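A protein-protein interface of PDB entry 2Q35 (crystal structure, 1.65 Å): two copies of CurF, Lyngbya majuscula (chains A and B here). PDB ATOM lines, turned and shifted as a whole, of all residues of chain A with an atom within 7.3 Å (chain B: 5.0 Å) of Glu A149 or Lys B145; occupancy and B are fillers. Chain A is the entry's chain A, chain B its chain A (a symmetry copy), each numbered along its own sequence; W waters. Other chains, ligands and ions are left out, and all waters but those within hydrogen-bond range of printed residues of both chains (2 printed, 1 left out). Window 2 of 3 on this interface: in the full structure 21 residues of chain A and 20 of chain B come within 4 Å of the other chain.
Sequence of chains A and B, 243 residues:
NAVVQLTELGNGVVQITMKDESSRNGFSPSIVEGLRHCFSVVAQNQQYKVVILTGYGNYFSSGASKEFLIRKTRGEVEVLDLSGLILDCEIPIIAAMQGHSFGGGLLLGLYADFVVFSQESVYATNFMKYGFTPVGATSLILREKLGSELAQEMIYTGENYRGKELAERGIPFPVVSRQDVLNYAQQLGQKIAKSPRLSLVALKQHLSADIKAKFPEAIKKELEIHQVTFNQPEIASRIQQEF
Of the 13 printed residues of chain A, 3 touch a printed residue of chain B. Hydrophobic or aromatic side chains of chain B within 4 Å of the printed part of chain A: Phe B173. Among the printed residues, 5 pairs touch across the chains. Among the printed residues, no Asp or Glu carboxylate lies within 4 Å of a Lys or Arg side-chain nitrogen of the other chain.
4 positions are printed for both chains.
Water W1 lies within hydrogen-bond range of OD1 of Asp B113 (2.8 Å) and NE2 of Gln A152 (2.8 Å). Water W2 lies within hydrogen-bond range of the backbone carbonyl oxygen (O) of Asp B113 and the side-chain carboxylate (OE2) of Glu A149.
The backbone carbonyl oxygen of Glu B144 sits at hydrogen-bond distance from the side-chain hydroxyl of Ser A148, at 3.4 Å. The side-chain amide nitrogen of Gln A152 lies within hydrogen-bond range of the backbone carbonyl oxygen of Asp B113 (3.3 Å). The backbone carbonyl oxygen of Lys B145 sits close to the side-chain carboxylate of Glu A149 (2.9 Å).
Glu A149 touches just these residues of chain B: Lys B145 (2.9 Å), Pro B172 (3.1 Å) and Phe B173 (3.3 Å). Of the printed residues of chain A, Phe B173 touches Glu A149. Printed residues of chain A within 4 Å of Pro B172: Glu A149. Printed residues of chain B within 4 Å of Gln A152: Asp B113 (3.3 Å). Ala B112 touches none of the printed residues of chain A. Glu A153 touches none of the printed residues of chain B. The nearest residue of chain A that does not touch Lys B145 is Ser A148 (4.9 Å).
Pro B172 touches Glu A149. Phe B173 touches Glu A149 (CZ to OE1, 3.3 Å).
The backbone carbonyl oxygen of Leu B110 lies within hydrogen-bond range of the side-chain amino group of Lys B145, at 2.9 Å. The backbone carbonyl oxygen (O) of Ala B112 is in hydrogen-bond range of the side-chain amino group (NZ) of Lys B145.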
ATOM      1  N   LEU A 142     -13.265 -17.744  16.373  1.00  0.00           N
ATOM      2  CA  LEU A 142     -12.000 -17.473  15.666  1.00  0.00           C
ATOM      3  C   LEU A 142     -11.060 -16.548  16.422  1.00  0.00           C
ATOM      4  O   LEU A 142      -9.846 -16.775  16.435  1.00  0.00           O
ATOM      5  CB  LEU A 142     -12.266 -16.917  14.270  1.00  0.00           C
ATOM      6  CG  LEU A 142     -12.144 -18.017  13.218  1.00  0.00           C
ATOM      7  CD1 LEU A 142     -13.376 -18.935  13.198  1.00  0.00           C
ATOM      8  CD2 LEU A 142     -11.866 -17.383  11.854  1.00  0.00           C
ATOM      9  N   ARG A 143     -11.595 -15.507  17.047  1.00  0.00           N
ATOM     10  CA  ARG A 143     -10.749 -14.586  17.800  1.00  0.00           C
ATOM     11  C   ARG A 143     -10.119 -15.294  18.988  1.00  0.00           C
ATOM     12  O   ARG A 143      -8.939 -15.093  19.274  1.00  0.00           O
ATOM     13  CB  ARG A 143     -11.510 -13.323  18.227  1.00  0.00           C
ATOM     14  CG  ARG A 143     -11.924 -12.515  17.018  1.00  0.00           C
ATOM     15  CD  ARG A 143     -12.140 -11.051  17.291  1.00  0.00           C
ATOM     16  NE  ARG A 143     -13.481 -10.764  17.785  1.00  0.00           N
ATOM     17  CZ  ARG A 143     -14.007  -9.540  17.807  1.00  0.00           C
ATOM     18  NH1 ARG A 143     -13.305  -8.511  17.352  1.00  0.00           N
ATOM     19  NH2 ARG A 143     -15.229  -9.342  18.284  1.00  0.00           N
ATOM     20  N   LEU A 146      -7.797 -18.582  16.923  1.00  0.00           N
ATOM     21  CA  LEU A 146      -6.767 -18.258  15.911  1.00  0.00           C
ATOM     22  C   LEU A 146      -6.037 -16.955  16.213  1.00  0.00           C
ATOM     23  O   LEU A 146      -4.992 -16.680  15.621  1.00  0.00           O
ATOM     24  CB  LEU A 146      -7.366 -18.178  14.505  1.00  0.00           C
ATOM     25  CG  LEU A 146      -8.201 -19.340  13.985  1.00  0.00           C
ATOM     26  CD1 LEU A 146      -8.588 -19.097  12.530  1.00  0.00           C
ATOM     27  CD2 LEU A 146      -7.476 -20.682  14.145  1.00  0.00           C
ATOM     28  N   GLY A 147      -6.596 -16.152  17.113  1.00  0.00           N
ATOM     29  CA  GLY A 147      -6.084 -14.813  17.408  1.00  0.00           C
ATOM     30  C   GLY A 147      -6.853 -13.756  16.640  1.00  0.00           C
ATOM     31  O   GLY A 147      -7.329 -14.023  15.541  1.00  0.00           O
ATOM     32  N   SER A 148      -6.976 -12.556  17.211  1.00  0.00           N
ATOM     33  CA  SER A 148      -7.836 -11.516  16.623  1.00  0.00           C
ATOM     34  C   SER A 148      -7.473 -11.114  15.180  1.00  0.00           C
ATOM     35  O   SER A 148      -8.372 -10.811  14.383  1.00  0.00           O
ATOM     36  CB  SER A 148      -7.949 -10.284  17.550  1.00  0.00           C
ATOM     37  OG  SER A 148      -6.679  -9.692  17.807  1.00  0.00           O
ATOM     38  N   GLU A 149      -6.187 -11.150  14.828  1.00  0.00           N
ATOM     39  CA  GLU A 149      -5.760 -10.709  13.489  1.00  0.00           C
ATOM     40  C   GLU A 149      -5.975 -11.673  12.338  1.00  0.00           C
ATOM     41  O   GLU A 149      -6.451 -11.257  11.280  1.00  0.00           O
ATOM     42  CB  GLU A 149      -4.316 -10.239  13.491  1.00  0.00           C
ATOM     43  CG  GLU A 149      -4.217  -8.745  13.466  1.00  0.00           C
ATOM     44  CD  GLU A 149      -4.642  -8.106  14.776  1.00  0.00           C
ATOM     45  OE1 GLU A 149      -3.810  -8.145  15.718  1.00  0.00           O
ATOM     46  OE2 GLU A 149      -5.777  -7.547  14.835  1.00  0.00           O
ATOM     47  N   LEU A 150      -5.616 -12.943  12.521  1.00  0.00           N
ATOM     48  CA  LEU A 150      -6.002 -13.950  11.543  1.00  0.00           C
ATOM     49  C   LEU A 150      -7.510 -13.980  11.458  1.00  0.00           C
ATOM     50  O   LEU A 150      -8.064 -14.054  10.372  1.00  0.00           O
ATOM     51  CB  LEU A 150      -5.496 -15.365  11.892  1.00  0.00           C
ATOM     52  CG  LEU A 150      -4.332 -15.956  11.081  1.00  0.00           C
ATOM     53  CD1 LEU A 150      -4.136 -17.419  11.452  1.00  0.00           C
ATOM     54  CD2 LEU A 150      -4.476 -15.806   9.563  1.00  0.00           C
ATOM     55  N   ALA A 151      -8.174 -13.947  12.613  1.00  0.00           N
ATOM     56  CA  ALA A 151      -9.627 -14.020  12.613  1.00  0.00           C
ATOM     57  C   ALA A 151     -10.189 -12.888  11.742  1.00  0.00           C
ATOM     58  O   ALA A 151     -11.021 -13.134  10.874  1.00  0.00           O
ATOM     59  CB  ALA A 151     -10.171 -13.948  14.043  1.00  0.00           C
ATOM     60  N   GLN A 152      -9.709 -11.668  11.972  1.00  0.00           N
ATOM     61  CA  GLN A 152     -10.144 -10.478  11.211  1.00  0.00           C
ATOM     62  C   GLN A 152      -9.983 -10.686   9.700  1.00  0.00           C
ATOM     63  O   GLN A 152     -10.909 -10.489   8.901  1.00  0.00           O
ATOM     64  CB  GLN A 152      -9.272  -9.292  11.637  1.00  0.00           C
ATOM     65  CG  GLN A 152      -9.793  -7.948  11.290  1.00  0.00           C
ATOM     66  CD  GLN A 152     -10.617  -7.340  12.400  1.00  0.00           C
ATOM     67  OE1 GLN A 152     -11.169  -8.043  13.246  1.00  0.00           O
ATOM     68  NE2 GLN A 152     -10.703  -6.033  12.401  1.00  0.00           N
ATOM     69  N   GLU A 153      -8.803 -11.107   9.292  1.00  0.00           N
ATOM     70  CA  GLU A 153      -8.562 -11.181   7.855  1.00  0.00           C
ATOM     71  C   GLU A 153      -9.360 -12.306   7.198  1.00  0.00           C
ATOM     72  O   GLU A 153      -9.923 -12.115   6.113  1.00  0.00           O
ATOM     73  CB  GLU A 153      -7.080 -11.336   7.549  1.00  0.00           C
ATOM     74  CG  GLU A 153      -6.793 -11.176   6.059  1.00  0.00           C
ATOM     75  CD  GLU A 153      -5.368 -11.548   5.687  1.00  0.00           C
ATOM     76  OE1 GLU A 153      -4.440 -10.865   6.155  1.00  0.00           O
ATOM     77  OE2 GLU A 153      -5.173 -12.514   4.917  1.00  0.00           O
ATOM     78  N   MET A 154      -9.398 -13.468   7.840  1.00  0.00           N
ATOM     79  CA  MET A 154     -10.143 -14.592   7.280  1.00  0.00           C
ATOM     80  C   MET A 154     -11.639 -14.271   7.174  1.00  0.00           C
ATOM     81  O   MET A 154     -12.269 -14.581   6.180  1.00  0.00           O
ATOM     82  CB  MET A 154      -9.946 -15.868   8.106  1.00  0.00           C
ATOM     83  CG  MET A 154      -8.521 -16.395   8.072  1.00  0.00           C
ATOM     84  SD  MET A 154      -8.363 -17.937   8.965  1.00  0.00           S
ATOM     85  CE  MET A 154      -9.214 -19.043   7.870  1.00  0.00           C
ATOM     86  N   ILE A 155     -12.180 -13.604   8.187  1.00  0.00           N
ATOM     87  CA  ILE A 155     -13.626 -13.298   8.189  1.00  0.00           C
ATOM     88  C   ILE A 155     -13.949 -12.217   7.145  1.00  0.00           C
ATOM     89  O   ILE A 155     -14.869 -12.368   6.338  1.00  0.00           O
ATOM     90  CB  ILE A 155     -14.104 -12.880   9.601  1.00  0.00           C
ATOM     91  CG1 ILE A 155     -13.939 -14.055  10.569  1.00  0.00           C
ATOM     92  CG2 ILE A 155     -15.573 -12.453   9.590  1.00  0.00           C
ATOM     93  CD1 ILE A 155     -14.222 -13.707  12.034  1.00  0.00           C
ATOM     94  N   ARG A 169       1.855 -17.613   9.034  1.00  0.00           N
ATOM     95  CA  ARG A 169       1.178 -16.486   9.642  1.00  0.00           C
ATOM     96  C   ARG A 169       1.165 -16.577  11.172  1.00  0.00           C
ATOM     97  O   ARG A 169       0.736 -15.648  11.854  1.00  0.00           O
ATOM     98  CB  ARG A 169      -0.259 -16.518   9.145  1.00  0.00           C
ATOM     99  CG  ARG A 169      -0.901 -15.215   8.975  1.00  0.00           C
ATOM    100  CD  ARG A 169      -0.408 -14.512   7.720  1.00  0.00           C
ATOM    101  NE  ARG A 169      -0.968 -13.177   7.761  1.00  0.00           N
ATOM    102  CZ  ARG A 169      -1.966 -12.742   7.003  1.00  0.00           C
ATOM    103  NH1 ARG A 169      -2.501 -13.510   6.057  1.00  0.00           N
ATOM    104  NH2 ARG A 169      -2.394 -11.503   7.177  1.00  0.00           N
ATOM    105  N   LEU B 110      -2.994   1.870  15.152  1.00  0.00           N
ATOM    106  CA  LEU B 110      -3.519   0.673  15.795  1.00  0.00           C
ATOM    107  C   LEU B 110      -5.031   0.739  16.050  1.00  0.00           C
ATOM    108  O   LEU B 110      -5.639  -0.298  16.362  1.00  0.00           O
ATOM    109  CB  LEU B 110      -2.765   0.357  17.103  1.00  0.00           C
ATOM    110  CG  LEU B 110      -1.317  -0.090  16.935  1.00  0.00           C
ATOM    111  CD1 LEU B 110      -0.688  -0.248  18.320  1.00  0.00           C
ATOM    112  CD2 LEU B 110      -1.247  -1.400  16.192  1.00  0.00           C
ATOM    113  N   TYR B 111      -5.610   1.928  15.882  1.00  0.00           N
ATOM    114  CA  TYR B 111      -7.083   2.093  16.021  1.00  0.00           C
ATOM    115  C   TYR B 111      -7.734   1.496  14.768  1.00  0.00           C
ATOM    116  O   TYR B 111      -8.927   1.178  14.770  1.00  0.00           O
ATOM    117  CB  TYR B 111      -7.511   3.564  16.137  1.00  0.00           C
ATOM    118  CG  TYR B 111      -7.129   4.275  17.426  1.00  0.00           C
ATOM    119  CD1 TYR B 111      -7.137   3.615  18.661  1.00  0.00           C
ATOM    120  CD2 TYR B 111      -6.782   5.632  17.392  1.00  0.00           C
ATOM    121  CE1 TYR B 111      -6.772   4.313  19.857  1.00  0.00           C
ATOM    122  CE2 TYR B 111      -6.437   6.327  18.548  1.00  0.00           C
ATOM    123  CZ  TYR B 111      -6.436   5.666  19.774  1.00  0.00           C
ATOM    124  OH  TYR B 111      -6.072   6.369  20.911  1.00  0.00           O
ATOM    125  N   ALA B 112      -6.939   1.315  13.697  1.00  0.00           N
ATOM    126  CA  ALA B 112      -7.490   0.803  12.433  1.00  0.00           C
ATOM    127  C   ALA B 112      -7.828  -0.689  12.524  1.00  0.00           C
ATOM    128  O   ALA B 112      -7.452  -1.393  13.464  1.00  0.00           O
ATOM    129  CB  ALA B 112      -6.511   1.054  11.254  1.00  0.00           C
ATOM    130  N   ASP B 113      -8.559  -1.175  11.533  1.00  0.00           N
ATOM    131  CA  ASP B 113      -8.986  -2.563  11.558  1.00  0.00           C
ATOM    132  C   ASP B 113      -7.884  -3.517  11.147  1.00  0.00           C
ATOM    133  O   ASP B 113      -7.811  -4.652  11.642  1.00  0.00           O
ATOM    134  CB  ASP B 113     -10.207  -2.727  10.674  1.00  0.00           C
ATOM    135  CG  ASP B 113     -11.310  -1.771  11.079  1.00  0.00           C
ATOM    136  OD1 ASP B 113     -11.948  -1.981  12.148  1.00  0.00           O
ATOM    137  OD2 ASP B 113     -11.485  -0.757  10.385  1.00  0.00           O
ATOM    138  N   ILE B 141      -5.699  -1.030  23.672  1.00  0.00           N
ATOM    139  CA  ILE B 141      -5.489  -1.277  22.244  1.00  0.00           C
ATOM    140  C   ILE B 141      -4.227  -2.116  22.003  1.00  0.00           C
ATOM    141  O   ILE B 141      -4.270  -3.079  21.230  1.00  0.00           O
ATOM    142  CB  ILE B 141      -5.493   0.046  21.456  1.00  0.00           C
ATOM    143  CG1 ILE B 141      -6.894   0.671  21.457  1.00  0.00           C
ATOM    144  CG2 ILE B 141      -5.062  -0.174  20.006  1.00  0.00           C
ATOM    145  CD1 ILE B 141      -7.994  -0.121  20.640  1.00  0.00           C
ATOM    146  N   LEU B 142      -3.120  -1.798  22.677  1.00  0.00           N
ATOM    147  CA  LEU B 142      -1.912  -2.609  22.437  1.00  0.00           C
ATOM    148  C   LEU B 142      -2.052  -4.061  22.867  1.00  0.00           C
ATOM    149  O   LEU B 142      -1.583  -4.961  22.165  1.00  0.00           O
ATOM    150  CB  LEU B 142      -0.695  -1.982  23.112  1.00  0.00           C
ATOM    151  CG  LEU B 142       0.134  -1.191  22.103  1.00  0.00           C
ATOM    152  CD1 LEU B 142      -0.506   0.166  21.767  1.00  0.00           C
ATOM    153  CD2 LEU B 142       1.565  -1.048  22.626  1.00  0.00           C
ATOM    154  N   ARG B 143      -2.684  -4.304  24.009  1.00  0.00           N
ATOM    155  CA  ARG B 143      -2.861  -5.676  24.472  1.00  0.00           C
ATOM    156  C   ARG B 143      -3.761  -6.447  23.521  1.00  0.00           C
ATOM    157  O   ARG B 143      -3.488  -7.606  23.211  1.00  0.00           O
ATOM    158  CB  ARG B 143      -3.378  -5.734  25.917  1.00  0.00           C
ATOM    159  CG  ARG B 143      -2.354  -5.168  26.874  1.00  0.00           C
ATOM    160  CD  ARG B 143      -2.473  -5.672  28.286  1.00  0.00           C
ATOM    161  NE  ARG B 143      -3.440  -4.918  29.072  1.00  0.00           N
ATOM    162  CZ  ARG B 143      -3.502  -4.970  30.402  1.00  0.00           C
ATOM    163  NH1 ARG B 143      -2.645  -5.727  31.075  1.00  0.00           N
ATOM    164  NH2 ARG B 143      -4.417  -4.270  31.061  1.00  0.00           N
ATOM    165  N   GLU B 144      -4.818  -5.798  23.038  1.00  0.00           N
ATOM    166  CA  GLU B 144      -5.725  -6.449  22.099  1.00  0.00           C
ATOM    167  C   GLU B 144      -5.023  -6.790  20.795  1.00  0.00           C
ATOM    168  O   GLU B 144      -5.178  -7.896  20.288  1.00  0.00           O
ATOM    169  CB  GLU B 144      -6.984  -5.601  21.853  1.00  0.00           C
ATOM    170  CG  GLU B 144      -7.911  -6.127  20.741  1.00  0.00           C
ATOM    171  CD  GLU B 144      -8.774  -7.316  21.168  1.00  0.00           C
ATOM    172  OE1 GLU B 144      -8.678  -7.773  22.335  1.00  0.00           O
ATOM    173  OE2 GLU B 144      -9.558  -7.802  20.311  1.00  0.00           O
ATOM    174  N   LYS B 145      -4.214  -5.874  20.292  1.00  0.00           N
ATOM    175  CA  LYS B 145      -3.736  -5.997  18.919  1.00  0.00           C
ATOM    176  C   LYS B 145      -2.316  -6.493  18.738  1.00  0.00           C
ATOM    177  O   LYS B 145      -2.046  -7.199  17.757  1.00  0.00           O
ATOM    178  CB  LYS B 145      -3.960  -4.707  18.167  1.00  0.00           C
ATOM    179  CG  LYS B 145      -5.405  -4.251  18.285  1.00  0.00           C
ATOM    180  CD  LYS B 145      -5.788  -3.445  17.104  1.00  0.00           C
ATOM    181  CE  LYS B 145      -7.227  -2.981  17.242  1.00  0.00           C
ATOM    182  NZ  LYS B 145      -7.607  -2.323  15.971  1.00  0.00           N
ATOM    183  N   LEU B 146      -1.419  -6.147  19.661  1.00  0.00           N
ATOM    184  CA  LEU B 146      -0.031  -6.653  19.580  1.00  0.00           C
ATOM    185  C   LEU B 146       0.202  -7.875  20.459  1.00  0.00           C
ATOM    186  O   LEU B 146       1.214  -8.562  20.310  1.00  0.00           O
ATOM    187  CB  LEU B 146       0.985  -5.571  19.957  1.00  0.00           C
ATOM    188  CG  LEU B 146       0.923  -4.219  19.258  1.00  0.00           C
ATOM    189  CD1 LEU B 146       2.095  -3.348  19.698  1.00  0.00           C
ATOM    190  CD2 LEU B 146       0.888  -4.364  17.731  1.00  0.00           C
ATOM    191  N   GLY B 147      -0.720  -8.131  21.381  1.00  0.00           N
ATOM    192  CA  GLY B 147      -0.569  -9.189  22.383  1.00  0.00           C
ATOM    193  C   GLY B 147      -0.051  -8.627  23.693  1.00  0.00           C
ATOM    194  O   GLY B 147       0.689  -7.649  23.688  1.00  0.00           O
ATOM    195  N   PRO B 172       1.596  -9.855  15.669  1.00  0.00           N
ATOM    196  CA  PRO B 172       0.572 -10.428  14.794  1.00  0.00           C
ATOM    197  C   PRO B 172       0.071  -9.483  13.707  1.00  0.00           C
ATOM    198  O   PRO B 172      -1.143  -9.358  13.528  1.00  0.00           O
ATOM    199  CB  PRO B 172      -0.563 -10.761  15.760  1.00  0.00           C
ATOM    200  CG  PRO B 172      -0.381  -9.830  16.923  1.00  0.00           C
ATOM    201  CD  PRO B 172       1.035  -9.320  16.926  1.00  0.00           C
ATOM    202  N   PHE B 173       0.975  -8.787  13.031  1.00  0.00           N
ATOM    203  CA  PHE B 173       0.611  -7.975  11.864  1.00  0.00           C
ATOM    204  C   PHE B 173       1.676  -8.188  10.812  1.00  0.00           C
ATOM    205  O   PHE B 173       2.794  -8.562  11.160  1.00  0.00           O
ATOM    206  CB  PHE B 173       0.583  -6.488  12.203  1.00  0.00           C
ATOM    207  CG  PHE B 173      -0.611  -6.069  13.017  1.00  0.00           C
ATOM    208  CD1 PHE B 173      -1.866  -6.020  12.435  1.00  0.00           C
ATOM    209  CD2 PHE B 173      -0.468  -5.705  14.340  1.00  0.00           C
ATOM    210  CE1 PHE B 173      -2.978  -5.615  13.159  1.00  0.00           C
ATOM    211  CE2 PHE B 173      -1.575  -5.291  15.082  1.00  0.00           C
ATOM    212  CZ  PHE B 173      -2.827  -5.240  14.481  1.00  0.00           C
HETATM  213  O   HOH W   1     -13.102  -4.534  12.215  1.00  0.00           O
HETATM  214  O   HOH W   2      -6.223  -6.980  11.750  1.00  0.00           O
